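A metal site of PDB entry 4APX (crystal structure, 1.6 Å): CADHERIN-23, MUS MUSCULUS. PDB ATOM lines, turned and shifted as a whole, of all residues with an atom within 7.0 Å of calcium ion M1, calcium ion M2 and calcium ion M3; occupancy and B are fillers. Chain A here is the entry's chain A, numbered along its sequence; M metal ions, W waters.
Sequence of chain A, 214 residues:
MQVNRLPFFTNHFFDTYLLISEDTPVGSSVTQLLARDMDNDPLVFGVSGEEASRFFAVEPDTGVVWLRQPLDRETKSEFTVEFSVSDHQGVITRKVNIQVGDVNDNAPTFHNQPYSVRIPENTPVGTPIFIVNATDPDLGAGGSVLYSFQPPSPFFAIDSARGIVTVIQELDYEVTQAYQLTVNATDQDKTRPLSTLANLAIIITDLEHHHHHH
The backbone NH (N) of Glu 22 sits at hydrogen-bond distance from the backbone carbonyl oxygen (O) of Gly 101 (2.9 Å).
OE1 of Glu 74 sits close to ND2 of Asn 106.
The backbone carbonyl oxygen of Asp 138 sits close to the backbone NH of Gly 143 (3.5 Å).
N of Asp 189 is in hydrogen-bond range of OD1 of Asp 187 (3.3 Å).
The backbone carbonyl oxygen (O) of Arg 192 is in hydrogen-bond range of the side-chain amide nitrogen (ND2) of Asn 104 (2.8 Å).
OD2 of Asp 72 sits at hydrogen-bond distance from OG1 of Thr 75, 2.6 Å away.
OD1 of Asp 105 sits close to ND2 of Asn 106 (3.1 Å).
The side-chain carboxylate (OD2) of Asp 102 sits at hydrogen-bond distance from the backbone NH (N) of Leu 139.
Six residues have an atom within 4 Å of calcium ion M3: Asn 104, Asn 106, Asp 136, Asp 138, Gly 142 and Asp 187.
Calcium ion M3 is bound by the backbone carbonyl oxygen (O) of Asn 106 (2.3 Å), the backbone carbonyl oxygen (O) of Gly 142 (2.3 Å), the side-chain carboxylate (OD2) of Asp 136 (2.4 Å), the side-chain amide oxygen (OD1) of Asn 104 (2.4 Å), the side-chain carboxylate (OD2) of Asp 187 (2.4 Å), the side-chain carboxylate (OD2) of Asp 138 (2.4 Å) and the side-chain carboxylate (OD1) of Asp 136 (2.5 Å).
Calcium ion M3 has seven donor atoms within binding distance.
Calcium ion M1 is bound by OD1 of Asp 138 (2.3 Å), OD1 of Asp 102 (2.3 Å), OE2 of Glu 22 (2.4 Å), OD1 of Asp 105 (2.4 Å), O of Val 103 (2.4 Å), OE2 of Glu 74 (2.4 Å) and OE1 of Glu 74 (2.6 Å).
Calcium ion M1 has seven donor atoms within binding distance.
Six residues have an atom within 4 Å of calcium ion M1: Glu 22, Glu 74, Asp 102, Val 103, Asp 105 and Asp 138.
Within 4 Å of calcium ion M2: Glu 22, Asp 72, Glu 74 and Asp 105.
The nearest printed residue that does not touch calcium ion M2 is Arg 73 (4.1 Å).
Calcium ion M2 is bound by OE1 of Glu 74 (2.3 Å), OD1 of Asp 72 (2.4 Å), OE1 of Glu 22 (2.4 Å), OD2 of Asp 105 (2.4 Å), water W1 (2.4 Å) and water W2 (2.4 Å).
Slightly farther from calcium ion M2 lies the side-chain carboxylate (OD1) of Asp 105 (2.9 Å).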
ATOM      1  N   GLU A  22     -19.022  -9.653  17.553  1.00  0.00           N
ATOM      2  CA  GLU A  22     -17.872 -10.532  17.266  1.00  0.00           C
ATOM      3  C   GLU A  22     -16.508  -9.991  17.724  1.00  0.00           C
ATOM      4  O   GLU A  22     -15.568 -10.775  17.804  1.00  0.00           O
ATOM      5  CB  GLU A  22     -17.799 -10.919  15.769  1.00  0.00           C
ATOM      6  CG  GLU A  22     -17.506  -9.781  14.851  1.00  0.00           C
ATOM      7  CD  GLU A  22     -17.287 -10.214  13.422  1.00  0.00           C
ATOM      8  OE1 GLU A  22     -16.804 -11.377  13.211  1.00  0.00           O
ATOM      9  OE2 GLU A  22     -17.554  -9.386  12.516  1.00  0.00           O
ATOM     10  N   LEU A  71     -15.339 -15.019  18.917  1.00  0.00           N
ATOM     11  CA  LEU A  71     -16.479 -15.227  18.045  1.00  0.00           C
ATOM     12  C   LEU A  71     -16.063 -14.746  16.656  1.00  0.00           C
ATOM     13  O   LEU A  71     -15.068 -14.023  16.505  1.00  0.00           O
ATOM     14  CB  LEU A  71     -17.706 -14.458  18.539  1.00  0.00           C
ATOM     15  CG  LEU A  71     -18.335 -14.887  19.865  1.00  0.00           C
ATOM     16  CD1 LEU A  71     -19.377 -13.871  20.308  1.00  0.00           C
ATOM     17  CD2 LEU A  71     -18.947 -16.268  19.795  1.00  0.00           C
ATOM     18  N   ASP A  72     -16.748 -15.212  15.630  1.00  0.00           N
ATOM     19  CA  ASP A  72     -16.470 -14.766  14.256  1.00  0.00           C
ATOM     20  C   ASP A  72     -17.747 -14.916  13.481  1.00  0.00           C
ATOM     21  O   ASP A  72     -18.104 -16.022  13.091  1.00  0.00           O
ATOM     22  CB  ASP A  72     -15.327 -15.576  13.613  1.00  0.00           C
ATOM     23  CG  ASP A  72     -15.112 -15.215  12.156  1.00  0.00           C
ATOM     24  OD1 ASP A  72     -15.645 -14.168  11.699  1.00  0.00           O
ATOM     25  OD2 ASP A  72     -14.415 -15.962  11.461  1.00  0.00           O
ATOM     26  N   ARG A  73     -18.416 -13.787  13.222  1.00  0.00           N
ATOM     27  CA  ARG A  73     -19.687 -13.780  12.554  1.00  0.00           C
ATOM     28  C   ARG A  73     -19.607 -14.402  11.157  1.00  0.00           C
ATOM     29  O   ARG A  73     -20.575 -14.993  10.680  1.00  0.00           O
ATOM     30  CB  ARG A  73     -20.234 -12.363  12.430  1.00  0.00           C
ATOM     31  CG  ARG A  73     -21.708 -12.319  12.021  1.00  0.00           C
ATOM     32  CD  ARG A  73     -22.135 -11.041  11.422  1.00  0.00           C
ATOM     33  NE  ARG A  73     -21.459 -10.857  10.130  1.00  0.00           N
ATOM     34  CZ  ARG A  73     -21.879 -11.343   8.968  1.00  0.00           C
ATOM     35  NH1 ARG A  73     -23.027 -12.006   8.843  1.00  0.00           N
ATOM     36  NH2 ARG A  73     -21.138 -11.130   7.893  1.00  0.00           N
ATOM     37  N   GLU A  74     -18.445 -14.253  10.516  1.00  0.00           N
ATOM     38  CA  GLU A  74     -18.230 -14.820   9.182  1.00  0.00           C
ATOM     39  C   GLU A  74     -17.994 -16.342   9.209  1.00  0.00           C
ATOM     40  O   GLU A  74     -18.075 -16.991   8.139  1.00  0.00           O
ATOM     41  CB  GLU A  74     -17.064 -14.123   8.490  1.00  0.00           C
ATOM     42  CG  GLU A  74     -17.378 -12.745   7.939  1.00  0.00           C
ATOM     43  CD  GLU A  74     -17.498 -11.661   9.005  1.00  0.00           C
ATOM     44  OE1 GLU A  74     -16.682 -11.595   9.949  1.00  0.00           O
ATOM     45  OE2 GLU A  74     -18.366 -10.773   8.839  1.00  0.00           O
ATOM     46  N   THR A  75     -17.672 -16.908  10.376  1.00  0.00           N
ATOM     47  CA  THR A  75     -17.469 -18.378  10.529  1.00  0.00           C
ATOM     48  C   THR A  75     -18.742 -19.009  11.109  1.00  0.00           C
ATOM     49  O   THR A  75     -19.162 -20.096  10.676  1.00  0.00           O
ATOM     50  CB  THR A  75     -16.238 -18.714  11.401  1.00  0.00           C
ATOM     51  OG1 THR A  75     -15.048 -18.405  10.663  1.00  0.00           O
ATOM     52  CG2 THR A  75     -16.192 -20.192  11.754  1.00  0.00           C
ATOM     53  N   GLY A 101     -22.977 -10.207  16.551  1.00  0.00           N
ATOM     54  CA  GLY A 101     -23.025  -8.914  15.891  1.00  0.00           C
ATOM     55  C   GLY A 101     -21.817  -8.717  14.994  1.00  0.00           C
ATOM     56  O   GLY A 101     -20.716  -9.178  15.308  1.00  0.00           O
ATOM     57  N   ASP A 102     -22.016  -8.040  13.876  1.00  0.00           N
ATOM     58  CA  ASP A 102     -20.931  -7.842  12.926  1.00  0.00           C
ATOM     59  C   ASP A 102     -20.084  -6.628  13.245  1.00  0.00           C
ATOM     60  O   ASP A 102     -20.586  -5.621  13.762  1.00  0.00           O
ATOM     61  CB  ASP A 102     -21.488  -7.659  11.499  1.00  0.00           C
ATOM     62  CG  ASP A 102     -20.406  -7.700  10.440  1.00  0.00           C
ATOM     63  OD1 ASP A 102     -19.613  -8.680  10.407  1.00  0.00           O
ATOM     64  OD2 ASP A 102     -20.319  -6.768   9.621  1.00  0.00           O
ATOM     65  N   VAL A 103     -18.799  -6.744  12.954  1.00  0.00           N
ATOM     66  CA  VAL A 103     -17.936  -5.584  12.851  1.00  0.00           C
ATOM     67  C   VAL A 103     -17.211  -5.705  11.525  1.00  0.00           C
ATOM     68  O   VAL A 103     -17.127  -6.789  10.962  1.00  0.00           O
ATOM     69  CB  VAL A 103     -16.978  -5.413  14.004  1.00  0.00           C
ATOM     70  CG1 VAL A 103     -17.711  -5.409  15.353  1.00  0.00           C
ATOM     71  CG2 VAL A 103     -15.915  -6.494  13.983  1.00  0.00           C
ATOM     72  N   ASN A 104     -16.727  -4.595  10.997  1.00  0.00           N
ATOM     73  CA  ASN A 104     -15.959  -4.653   9.751  1.00  0.00           C
ATOM     74  C   ASN A 104     -14.583  -5.209  10.071  1.00  0.00           C
ATOM     75  O   ASN A 104     -13.740  -4.508  10.634  1.00  0.00           O
ATOM     76  CB  ASN A 104     -15.860  -3.274   9.079  1.00  0.00           C
ATOM     77  CG  ASN A 104     -15.250  -3.373   7.709  1.00  0.00           C
ATOM     78  OD1 ASN A 104     -15.702  -4.204   6.924  1.00  0.00           O
ATOM     79  ND2 ASN A 104     -14.201  -2.610   7.432  1.00  0.00           N
ATOM     80  N   ASP A 105     -14.379  -6.487   9.752  1.00  0.00           N
ATOM     81  CA  ASP A 105     -13.081  -7.109  10.038  1.00  0.00           C
ATOM     82  C   ASP A 105     -12.473  -7.878   8.880  1.00  0.00           C
ATOM     83  O   ASP A 105     -11.452  -8.571   9.067  1.00  0.00           O
ATOM     84  CB  ASP A 105     -13.096  -7.920  11.356  1.00  0.00           C
ATOM     85  CG  ASP A 105     -14.107  -9.050  11.390  1.00  0.00           C
ATOM     86  OD1 ASP A 105     -14.958  -9.160  10.490  1.00  0.00           O
ATOM     87  OD2 ASP A 105     -14.057  -9.874  12.353  1.00  0.00           O
ATOM     88  N   ASN A 106     -13.041  -7.726   7.678  1.00  0.00           N
ATOM     89  CA  ASN A 106     -12.485  -8.283   6.470  1.00  0.00           C
ATOM     90  C   ASN A 106     -12.233  -7.213   5.423  1.00  0.00           C
ATOM     91  O   ASN A 106     -13.020  -6.287   5.269  1.00  0.00           O
ATOM     92  CB  ASN A 106     -13.412  -9.341   5.832  1.00  0.00           C
ATOM     93  CG  ASN A 106     -13.586 -10.549   6.707  1.00  0.00           C
ATOM     94  OD1 ASN A 106     -12.881 -11.563   6.511  1.00  0.00           O
ATOM     95  ND2 ASN A 106     -14.477 -10.467   7.709  1.00  0.00           N
ATOM     96  N   ALA A 107     -11.138  -7.376   4.697  1.00  0.00           N
ATOM     97  CA  ALA A 107     -10.863  -6.561   3.536  1.00  0.00           C
ATOM     98  C   ALA A 107     -11.431  -7.295   2.330  1.00  0.00           C
ATOM     99  O   ALA A 107     -11.663  -8.514   2.390  1.00  0.00           O
ATOM    100  CB  ALA A 107      -9.371  -6.309   3.351  1.00  0.00           C
ATOM    101  N   PRO A 108     -11.668  -6.570   1.217  1.00  0.00           N
ATOM    102  CA  PRO A 108     -12.136  -7.262   0.013  1.00  0.00           C
ATOM    103  C   PRO A 108     -11.136  -8.263  -0.571  1.00  0.00           C
ATOM    104  O   PRO A 108      -9.926  -8.162  -0.343  1.00  0.00           O
ATOM    105  CB  PRO A 108     -12.381  -6.127  -0.987  1.00  0.00           C
ATOM    106  CG  PRO A 108     -12.568  -4.903  -0.111  1.00  0.00           C
ATOM    107  CD  PRO A 108     -11.660  -5.105   1.035  1.00  0.00           C
ATOM    108  N   ASP A 136     -16.596  -8.857  -0.390  1.00  0.00           N
ATOM    109  CA  ASP A 136     -16.259  -8.612   1.008  1.00  0.00           C
ATOM    110  C   ASP A 136     -17.406  -9.105   1.861  1.00  0.00           C
ATOM    111  O   ASP A 136     -18.550  -8.677   1.639  1.00  0.00           O
ATOM    112  CB  ASP A 136     -16.034  -7.111   1.165  1.00  0.00           C
ATOM    113  CG  ASP A 136     -15.528  -6.701   2.557  1.00  0.00           C
ATOM    114  OD1 ASP A 136     -15.994  -7.252   3.594  1.00  0.00           O
ATOM    115  OD2 ASP A 136     -14.681  -5.777   2.629  1.00  0.00           O
ATOM    116  N   PRO A 137     -17.135 -10.008   2.822  1.00  0.00           N
ATOM    117  CA  PRO A 137     -18.189 -10.687   3.573  1.00  0.00           C
ATOM    118  C   PRO A 137     -18.832  -9.953   4.733  1.00  0.00           C
ATOM    119  O   PRO A 137     -19.818 -10.444   5.286  1.00  0.00           O
ATOM    120  CB  PRO A 137     -17.468 -11.935   4.106  1.00  0.00           C
ATOM    121  CG  PRO A 137     -16.095 -11.460   4.370  1.00  0.00           C
ATOM    122  CD  PRO A 137     -15.806 -10.551   3.172  1.00  0.00           C
ATOM    123  N   ASP A 138     -18.297  -8.800   5.106  1.00  0.00           N
ATOM    124  CA  ASP A 138     -18.866  -8.041   6.212  1.00  0.00           C
ATOM    125  C   ASP A 138     -20.209  -7.474   5.818  1.00  0.00           C
ATOM    126  O   ASP A 138     -20.525  -7.383   4.628  1.00  0.00           O
ATOM    127  CB  ASP A 138     -17.929  -6.928   6.596  1.00  0.00           C
ATOM    128  CG  ASP A 138     -16.612  -7.432   7.181  1.00  0.00           C
ATOM    129  OD1 ASP A 138     -16.630  -8.193   8.179  1.00  0.00           O
ATOM    130  OD2 ASP A 138     -15.578  -7.032   6.645  1.00  0.00           O
ATOM    131  N   LEU A 139     -21.006  -7.091   6.808  1.00  0.00           N
ATOM    132  CA  LEU A 139     -22.349  -6.567   6.541  1.00  0.00           C
ATOM    133  C   LEU A 139     -22.365  -5.103   6.156  1.00  0.00           C
ATOM    134  O   LEU A 139     -21.477  -4.318   6.557  1.00  0.00           O
ATOM    135  CB  LEU A 139     -23.249  -6.738   7.775  1.00  0.00           C
ATOM    136  CG  LEU A 139     -23.574  -8.161   8.257  1.00  0.00           C
ATOM    137  CD1 LEU A 139     -24.552  -8.162   9.429  1.00  0.00           C
ATOM    138  CD2 LEU A 139     -24.117  -8.978   7.102  1.00  0.00           C
ATOM    139  N   ALA A 141     -22.216  -1.415   4.904  1.00  0.00           N
ATOM    140  CA  ALA A 141     -21.171  -0.606   4.270  1.00  0.00           C
ATOM    141  C   ALA A 141     -19.835  -1.318   4.272  1.00  0.00           C
ATOM    142  O   ALA A 141     -19.048  -1.186   3.335  1.00  0.00           O
ATOM    143  CB  ALA A 141     -21.058   0.753   4.964  1.00  0.00           C
ATOM    144  N   GLY A 142     -19.580  -2.088   5.315  1.00  0.00           N
ATOM    145  CA  GLY A 142     -18.380  -2.923   5.408  1.00  0.00           C
ATOM    146  C   GLY A 142     -18.234  -3.994   4.360  1.00  0.00           C
ATOM    147  O   GLY A 142     -17.145  -4.542   4.198  1.00  0.00           O
ATOM    148  N   GLY A 143     -19.307  -4.305   3.629  1.00  0.00           N
ATOM    149  CA  GLY A 143     -19.276  -5.280   2.569  1.00  0.00           C
ATOM    150  C   GLY A 143     -19.479  -4.732   1.176  1.00  0.00           C
ATOM    151  O   GLY A 143     -19.563  -5.499   0.215  1.00  0.00           O
ATOM    152  N   SER A 144     -19.592  -3.408   1.051  1.00  0.00           N
ATOM    153  CA  SER A 144     -19.865  -2.750  -0.234  1.00  0.00           C
ATOM    154  C   SER A 144     -18.566  -2.186  -0.749  1.00  0.00           C
ATOM    155  O   SER A 144     -17.954  -1.338  -0.105  1.00  0.00           O
ATOM    156  CB  SER A 144     -20.922  -1.662  -0.055  1.00  0.00           C
ATOM    157  OG  SER A 144     -21.258  -1.048  -1.294  1.00  0.00           O
ATOM    158  N   THR A 186     -11.836  -1.139  -1.845  1.00  0.00           N
ATOM    159  CA  THR A 186     -12.077  -0.813  -0.431  1.00  0.00           C
ATOM    160  C   THR A 186     -13.512  -1.021  -0.072  1.00  0.00           C
ATOM    161  O   THR A 186     -14.401  -0.836  -0.888  1.00  0.00           O
ATOM    162  CB  THR A 186     -11.682   0.660  -0.101  1.00  0.00           C
ATOM    163  OG1 THR A 186     -11.813   0.897   1.311  1.00  0.00           O
ATOM    164  CG2 THR A 186     -12.567   1.669  -0.865  1.00  0.00           C
ATOM    165  N   ASP A 187     -13.771  -1.433   1.170  1.00  0.00           N
ATOM    166  CA  ASP A 187     -15.123  -1.388   1.678  1.00  0.00           C
ATOM    167  C   ASP A 187     -15.408   0.061   2.112  1.00  0.00           C
ATOM    168  O   ASP A 187     -14.522   0.931   1.981  1.00  0.00           O
ATOM    169  CB  ASP A 187     -15.383  -2.420   2.783  1.00  0.00           C
ATOM    170  CG  ASP A 187     -14.564  -2.211   3.996  1.00  0.00           C
ATOM    171  OD1 ASP A 187     -14.377  -1.059   4.407  1.00  0.00           O
ATOM    172  OD2 ASP A 187     -14.119  -3.233   4.585  1.00  0.00           O
ATOM    173  N   GLN A 188     -16.632   0.309   2.574  1.00  0.00           N
ATOM    174  CA  GLN A 188     -17.073   1.655   2.933  1.00  0.00           C
ATOM    175  C   GLN A 188     -17.425   1.808   4.418  1.00  0.00           C
ATOM    176  O   GLN A 188     -18.223   2.663   4.796  1.00  0.00           O
ATOM    177  CB  GLN A 188     -18.264   2.042   2.061  1.00  0.00           C
ATOM    178  CG  GLN A 188     -17.884   2.158   0.603  1.00  0.00           C
ATOM    179  CD  GLN A 188     -19.061   2.448  -0.256  1.00  0.00           C
ATOM    180  OE1 GLN A 188     -19.463   3.612  -0.405  1.00  0.00           O
ATOM    181  NE2 GLN A 188     -19.650   1.392  -0.826  1.00  0.00           N
ATOM    182  N   ASP A 189     -16.800   1.016   5.262  1.00  0.00           N
ATOM    183  CA  ASP A 189     -17.033   1.111   6.683  1.00  0.00           C
ATOM    184  C   ASP A 189     -16.695   2.528   7.138  1.00  0.00           C
ATOM    185  O   ASP A 189     -15.699   3.098   6.711  1.00  0.00           O
ATOM    186  CB  ASP A 189     -16.222   0.119   7.488  1.00  0.00           C
ATOM    187  CG  ASP A 189     -16.595   0.136   8.951  1.00  0.00           C
ATOM    188  OD1 ASP A 189     -17.769  -0.197   9.277  1.00  0.00           O
ATOM    189  OD2 ASP A 189     -15.736   0.513   9.776  1.00  0.00           O
ATOM    190  N   ARG A 192     -13.561   2.201  10.217  1.00  0.00           N
ATOM    191  CA  ARG A 192     -12.419   1.315   9.950  1.00  0.00           C
ATOM    192  C   ARG A 192     -12.536   0.655   8.574  1.00  0.00           C
ATOM    193  O   ARG A 192     -12.633  -0.572   8.480  1.00  0.00           O
ATOM    194  CB  ARG A 192     -12.298   0.249  11.035  1.00  0.00           C
ATOM    195  CG  ARG A 192     -11.999   0.810  12.454  1.00  0.00           C
ATOM    196  CD  ARG A 192     -11.802  -0.268  13.520  1.00  0.00           C
ATOM    197  NE  ARG A 192     -10.758  -1.215  13.187  1.00  0.00           N
ATOM    198  CZ  ARG A 192     -10.924  -2.393  12.578  1.00  0.00           C
ATOM    199  NH1 ARG A 192     -12.140  -2.833  12.252  1.00  0.00           N
ATOM    200  NH2 ARG A 192      -9.863  -3.122  12.284  1.00  0.00           N
ATOM    201  N   PRO A 193     -12.499   1.458   7.515  1.00  0.00           N
ATOM    202  CA  PRO A 193     -12.524   0.879   6.183  1.00  0.00           C
ATOM    203  C   PRO A 193     -11.279   0.023   5.910  1.00  0.00           C
ATOM    204  O   PRO A 193     -10.189   0.366   6.359  1.00  0.00           O
ATOM    205  CB  PRO A 193     -12.541   2.093   5.275  1.00  0.00           C
ATOM    206  CG  PRO A 193     -11.785   3.141   6.082  1.00  0.00           C
ATOM    207  CD  PRO A 193     -12.314   2.926   7.458  1.00  0.00           C
ATOM    208  N   LEU A 194     -11.487  -1.078   5.213  1.00  0.00           N
ATOM    209  CA  LEU A 194     -10.425  -2.006   4.897  1.00  0.00           C
ATOM    210  C   LEU A 194     -10.330  -2.160   3.391  1.00  0.00           C
ATOM    211  O   LEU A 194     -11.338  -2.138   2.695  1.00  0.00           O
ATOM    212  CB  LEU A 194     -10.672  -3.348   5.572  1.00  0.00           C
ATOM    213  CG  LEU A 194     -10.637  -3.288   7.107  1.00  0.00           C
ATOM    214  CD1 LEU A 194     -11.076  -4.602   7.684  1.00  0.00           C
ATOM    215  CD2 LEU A 194      -9.261  -2.898   7.611  1.00  0.00           C
HETATM  216 CA    CA M   1     -17.338  -9.054  10.186  1.00  0.00          CA
HETATM  217 CA    CA M   2     -15.117 -11.872  11.633  1.00  0.00          CA
HETATM  218 CA    CA M   3     -15.095  -5.393   4.936  1.00  0.00          CA
HETATM  219  O   HOH W   1     -13.508 -12.329   9.932  1.00  0.00           O
HETATM  220  O   HOH W   2     -13.581 -12.717  13.265  1.00  0.00           O
